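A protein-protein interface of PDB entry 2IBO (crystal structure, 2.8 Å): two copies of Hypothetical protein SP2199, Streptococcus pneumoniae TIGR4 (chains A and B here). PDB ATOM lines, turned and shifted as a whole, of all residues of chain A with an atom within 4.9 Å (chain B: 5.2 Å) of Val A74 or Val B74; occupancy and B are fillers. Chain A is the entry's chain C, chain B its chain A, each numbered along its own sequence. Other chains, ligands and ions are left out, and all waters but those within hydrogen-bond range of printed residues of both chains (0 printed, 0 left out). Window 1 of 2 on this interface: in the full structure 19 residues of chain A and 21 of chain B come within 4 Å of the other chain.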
ATOM      1  N   ILE A   5      23.609  -5.640  -5.274  1.00  0.00           N
ATOM      2  CA  ILE A   5      23.643  -6.543  -6.431  1.00  0.00           C
ATOM      3  C   ILE A   5      25.023  -7.195  -6.450  1.00  0.00           C
ATOM      4  O   ILE A   5      26.012  -6.558  -6.080  1.00  0.00           O
ATOM      5  CB  ILE A   5      23.463  -5.722  -7.765  1.00  0.00           C
ATOM      6  CG1 ILE A   5      22.105  -5.032  -7.766  1.00  0.00           C
ATOM      7  CG2 ILE A   5      23.579  -6.595  -8.990  1.00  0.00           C
ATOM      8  CD1 ILE A   5      20.960  -5.977  -7.646  1.00  0.00           C
ATOM      9  N   ALA A   6      25.086  -8.461  -6.854  1.00  0.00           N
ATOM     10  CA  ALA A   6      26.350  -9.195  -6.979  1.00  0.00           C
ATOM     11  C   ALA A   6      26.265  -9.749  -8.396  1.00  0.00           C
ATOM     12  O   ALA A   6      25.456 -10.622  -8.672  1.00  0.00           O
ATOM     13  CB  ALA A   6      26.415 -10.317  -5.963  1.00  0.00           C
ATOM     14  N   LEU A   7      27.090  -9.237  -9.295  1.00  0.00           N
ATOM     15  CA  LEU A   7      27.038  -9.628 -10.705  1.00  0.00           C
ATOM     16  C   LEU A   7      28.117 -10.556 -11.255  1.00  0.00           C
ATOM     17  O   LEU A   7      29.306 -10.304 -11.089  1.00  0.00           O
ATOM     18  CB  LEU A   7      27.002  -8.364 -11.560  1.00  0.00           C
ATOM     19  CG  LEU A   7      27.358  -8.481 -13.042  1.00  0.00           C
ATOM     20  CD1 LEU A   7      26.379  -9.410 -13.760  1.00  0.00           C
ATOM     21  CD2 LEU A   7      27.349  -7.074 -13.649  1.00  0.00           C
ATOM     22  N   LEU A  56      22.947  -2.467 -13.902  1.00  0.00           N
ATOM     23  CA  LEU A  56      22.922  -3.881 -14.266  1.00  0.00           C
ATOM     24  C   LEU A  56      22.582  -4.028 -15.744  1.00  0.00           C
ATOM     25  O   LEU A  56      23.279  -4.731 -16.483  1.00  0.00           O
ATOM     26  CB  LEU A  56      21.879  -4.632 -13.435  1.00  0.00           C
ATOM     27  CG  LEU A  56      21.610  -6.107 -13.768  1.00  0.00           C
ATOM     28  CD1 LEU A  56      22.909  -6.919 -13.706  1.00  0.00           C
ATOM     29  CD2 LEU A  56      20.579  -6.662 -12.773  1.00  0.00           C
ATOM     30  N   ALA A  72      24.540 -14.524 -17.344  1.00  0.00           N
ATOM     31  CA  ALA A  72      24.934 -13.851 -16.117  1.00  0.00           C
ATOM     32  C   ALA A  72      24.154 -14.323 -14.904  1.00  0.00           C
ATOM     33  O   ALA A  72      22.972 -14.656 -14.993  1.00  0.00           O
ATOM     34  CB  ALA A  72      24.786 -12.350 -16.272  1.00  0.00           C
ATOM     35  N   ASN A  73      24.843 -14.375 -13.775  1.00  0.00           N
ATOM     36  CA  ASN A  73      24.252 -14.764 -12.508  1.00  0.00           C
ATOM     37  C   ASN A  73      24.159 -13.432 -11.798  1.00  0.00           C
ATOM     38  O   ASN A  73      25.127 -12.664 -11.793  1.00  0.00           O
ATOM     39  CB  ASN A  73      25.198 -15.662 -11.706  1.00  0.00           C
ATOM     40  CG  ASN A  73      25.193 -17.104 -12.170  1.00  0.00           C
ATOM     41  OD1 ASN A  73      26.209 -17.800 -12.070  1.00  0.00           O
ATOM     42  ND2 ASN A  73      24.048 -17.573 -12.653  1.00  0.00           N
ATOM     43  N   VAL A  74      23.014 -13.141 -11.204  1.00  0.00           N
ATOM     44  CA  VAL A  74      22.870 -11.889 -10.491  1.00  0.00           C
ATOM     45  C   VAL A  74      22.201 -12.150  -9.162  1.00  0.00           C
ATOM     46  O   VAL A  74      21.280 -12.966  -9.069  1.00  0.00           O
ATOM     47  CB  VAL A  74      22.009 -10.852 -11.274  1.00  0.00           C
ATOM     48  CG1 VAL A  74      22.023  -9.509 -10.522  1.00  0.00           C
ATOM     49  CG2 VAL A  74      22.557 -10.661 -12.692  1.00  0.00           C
ATOM     50  N   LYS A  75      22.682 -11.464  -8.133  1.00  0.00           N
ATOM     51  CA  LYS A  75      22.121 -11.573  -6.799  1.00  0.00           C
ATOM     52  C   LYS A  75      21.619 -10.194  -6.451  1.00  0.00           C
ATOM     53  O   LYS A  75      22.337  -9.209  -6.629  1.00  0.00           O
ATOM     54  CB  LYS A  75      23.186 -11.965  -5.784  1.00  0.00           C
ATOM     55  CG  LYS A  75      23.527 -13.432  -5.746  1.00  0.00           C
ATOM     56  CD  LYS A  75      24.723 -13.668  -4.833  1.00  0.00           C
ATOM     57  CE  LYS A  75      25.205 -15.104  -4.919  1.00  0.00           C
ATOM     58  NZ  LYS A  75      26.451 -15.291  -4.140  1.00  0.00           N
ATOM     59  N   ILE A  76      20.389 -10.111  -5.966  1.00  0.00           N
ATOM     60  CA  ILE A  76      19.828  -8.827  -5.584  1.00  0.00           C
ATOM     61  C   ILE A  76      19.391  -8.900  -4.138  1.00  0.00           C
ATOM     62  O   ILE A  76      18.800  -9.895  -3.708  1.00  0.00           O
ATOM     63  CB  ILE A  76      18.633  -8.461  -6.451  1.00  0.00           C
ATOM     64  CG1 ILE A  76      19.071  -8.413  -7.926  1.00  0.00           C
ATOM     65  CG2 ILE A  76      18.045  -7.128  -5.977  1.00  0.00           C
ATOM     66  CD1 ILE A  76      17.935  -8.202  -8.926  1.00  0.00           C
ATOM     67  N   ILE B   5      15.132 -14.607 -18.571  1.00  0.00           N
ATOM     68  CA  ILE B   5      15.365 -14.272 -17.173  1.00  0.00           C
ATOM     69  C   ILE B   5      14.756 -15.352 -16.306  1.00  0.00           C
ATOM     70  O   ILE B   5      13.617 -15.759 -16.525  1.00  0.00           O
ATOM     71  CB  ILE B   5      14.677 -12.917 -16.839  1.00  0.00           C
ATOM     72  CG1 ILE B   5      15.440 -11.786 -17.512  1.00  0.00           C
ATOM     73  CG2 ILE B   5      14.548 -12.709 -15.347  1.00  0.00           C
ATOM     74  CD1 ILE B   5      16.888 -11.754 -17.125  1.00  0.00           C
ATOM     75  N   ALA B   6      15.516 -15.833 -15.332  1.00  0.00           N
ATOM     76  CA  ALA B   6      15.021 -16.848 -14.413  1.00  0.00           C
ATOM     77  C   ALA B   6      14.980 -16.132 -13.073  1.00  0.00           C
ATOM     78  O   ALA B   6      15.970 -15.519 -12.659  1.00  0.00           O
ATOM     79  CB  ALA B   6      15.976 -18.022 -14.372  1.00  0.00           C
ATOM     80  N   LEU B   7      13.838 -16.163 -12.400  1.00  0.00           N
ATOM     81  CA  LEU B   7      13.732 -15.461 -11.118  1.00  0.00           C
ATOM     82  C   LEU B   7      13.314 -16.353  -9.954  1.00  0.00           C
ATOM     83  O   LEU B   7      12.416 -17.204 -10.079  1.00  0.00           O
ATOM     84  CB  LEU B   7      12.750 -14.277 -11.237  1.00  0.00           C
ATOM     85  CG  LEU B   7      12.466 -13.437  -9.973  1.00  0.00           C
ATOM     86  CD1 LEU B   7      13.739 -12.652  -9.544  1.00  0.00           C
ATOM     87  CD2 LEU B   7      11.302 -12.487 -10.247  1.00  0.00           C
ATOM     88  N   LEU B  56      11.544  -7.476 -14.297  1.00  0.00           N
ATOM     89  CA  LEU B  56      12.368  -7.918 -13.170  1.00  0.00           C
ATOM     90  C   LEU B  56      12.327  -6.869 -12.068  1.00  0.00           C
ATOM     91  O   LEU B  56      12.079  -7.194 -10.904  1.00  0.00           O
ATOM     92  CB  LEU B  56      13.826  -8.141 -13.607  1.00  0.00           C
ATOM     93  CG  LEU B  56      14.867  -8.481 -12.515  1.00  0.00           C
ATOM     94  CD1 LEU B  56      14.462  -9.753 -11.755  1.00  0.00           C
ATOM     95  CD2 LEU B  56      16.236  -8.663 -13.149  1.00  0.00           C
ATOM     96  N   ALA B  72      17.060 -12.160  -3.909  1.00  0.00           N
ATOM     97  CA  ALA B  72      16.674 -12.815  -5.144  1.00  0.00           C
ATOM     98  C   ALA B  72      17.857 -13.323  -5.932  1.00  0.00           C
ATOM     99  O   ALA B  72      18.923 -12.718  -5.933  1.00  0.00           O
ATOM    100  CB  ALA B  72      15.848 -11.847  -6.010  1.00  0.00           C
ATOM    101  N   ASN B  73      17.656 -14.457  -6.594  1.00  0.00           N
ATOM    102  CA  ASN B  73      18.670 -15.050  -7.444  1.00  0.00           C
ATOM    103  C   ASN B  73      18.092 -14.784  -8.805  1.00  0.00           C
ATOM    104  O   ASN B  73      16.910 -15.036  -9.019  1.00  0.00           O
ATOM    105  CB  ASN B  73      18.751 -16.569  -7.253  1.00  0.00           C
ATOM    106  CG  ASN B  73      19.571 -16.982  -6.040  1.00  0.00           C
ATOM    107  OD1 ASN B  73      19.297 -18.020  -5.424  1.00  0.00           O
ATOM    108  ND2 ASN B  73      20.588 -16.199  -5.703  1.00  0.00           N
ATOM    109  N   VAL B  74      18.897 -14.271  -9.722  1.00  0.00           N
ATOM    110  CA  VAL B  74      18.402 -14.032 -11.063  1.00  0.00           C
ATOM    111  C   VAL B  74      19.412 -14.561 -12.056  1.00  0.00           C
ATOM    112  O   VAL B  74      20.617 -14.452 -11.835  1.00  0.00           O
ATOM    113  CB  VAL B  74      18.188 -12.526 -11.342  1.00  0.00           C
ATOM    114  CG1 VAL B  74      17.562 -12.344 -12.713  1.00  0.00           C
ATOM    115  CG2 VAL B  74      17.300 -11.921 -10.277  1.00  0.00           C
ATOM    116  N   LYS B  75      18.914 -15.155 -13.134  1.00  0.00           N
ATOM    117  CA  LYS B  75      19.762 -15.666 -14.192  1.00  0.00           C
ATOM    118  C   LYS B  75      19.353 -14.897 -15.422  1.00  0.00           C
ATOM    119  O   LYS B  75      18.161 -14.778 -15.721  1.00  0.00           O
ATOM    120  CB  LYS B  75      19.515 -17.149 -14.445  1.00  0.00           C
ATOM    121  CG  LYS B  75      20.190 -18.070 -13.487  1.00  0.00           C
ATOM    122  CD  LYS B  75      19.710 -19.491 -13.709  1.00  0.00           C
ATOM    123  CE  LYS B  75      20.226 -20.413 -12.622  1.00  0.00           C
ATOM    124  NZ  LYS B  75      19.613 -21.763 -12.756  1.00  0.00           N
ATOM    125  N   ILE B  76      20.333 -14.353 -16.121  1.00  0.00           N
ATOM    126  CA  ILE B  76      20.028 -13.634 -17.334  1.00  0.00           C
ATOM    127  C   ILE B  76      20.792 -14.298 -18.457  1.00  0.00           C
ATOM    128  O   ILE B  76      21.917 -14.772 -18.270  1.00  0.00           O
ATOM    129  CB  ILE B  76      20.415 -12.154 -17.212  1.00  0.00           C
ATOM    130  CG1 ILE B  76      19.811 -11.590 -15.910  1.00  0.00           C
ATOM    131  CG2 ILE B  76      19.944 -11.389 -18.457  1.00  0.00           C
ATOM    132  CD1 ILE B  76      19.901 -10.087 -15.737  1.00  0.00           C
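N of Val B74 lies within hydrogen-bond range of O of Val A74, 2.8 Å away.
O of Ile B76 sits at hydrogen-bond distance from N of Ala A72 (2.8 Å).
The backbone carbonyl oxygen (O) of Ile A76 sits at hydrogen-bond distance from the backbone NH (N) of Ala B72 (2.9 Å).
O of Lys B75 is in hydrogen-bond range of N of Ala B6 (2.9 Å).
O of Lys A75 sits at hydrogen-bond distance from N of Ala A6 (2.9 Å).
O of Ala A72 touches O of Val B74, at 3.9 Å.
Lys B75 touches Ala A72 (CA to O, 3.5 Å).
C of Asn A73 touches O of Val B74, 3.7 Å away.
ND2 of Asn A73 touches CG of Lys B75 (3.98 Å).
O of Val A74 touches O of Ala B72, 3.9 Å away.
O of Val A74 touches C of Asn B73, 3.7 Å away.
Lys A75 touches Ala B72.
Of the printed residues of chain B, Asn A73 touches Val B74 and Lys B75.
Of the printed residues of chain B, Val A74 touches Ala B72, Asn B73 and Val B74.
Of the printed residues of chain B, Ile A76 touches Ala B72 (2.9 Å).
Ala B6 touches none of the printed residues of chain A.
Of the printed residues of chain A, Ala B72 touches Val A74, Lys A75 and Ile A76.
Printed residues of chain A within 4 Å of Val B74: Ala A72 (3.9 Å), Asn A73 (3.7 Å) and Val A74 (2.8 Å).
Of the printed residues of chain A, Lys B75 touches Ala A72 and Asn A73.
Of the printed residues of chain A, Ile B76 touches Ala A72.
The nearest residue of chain B that does not touch Val A74 is Ile B76 (4.1 Å).
Of the 9 printed residues of chain B, 5 touch a printed residue of chain A.
Printed residues of chain B that touch a printed residue of chain A: Ala B72, Asn B73, Val B74, Lys B75 and Ile B76.
Of the 9 printed residues of chain A, 5 touch a printed residue of chain B.
Ala A72 touches Val B74, and with the chains exchanged Val A74 touches Ala B72.
Ala A72 touches Ile B76, and with the chains exchanged Ile A76 touches Ala B72.
Asn A73 touches Val B74, and with the chains exchanged Val A74 touches Asn B73.
Asn A73 touches Lys B75, but with the chains exchanged Lys A75 does not touch Asn B73 (4.04 Å).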
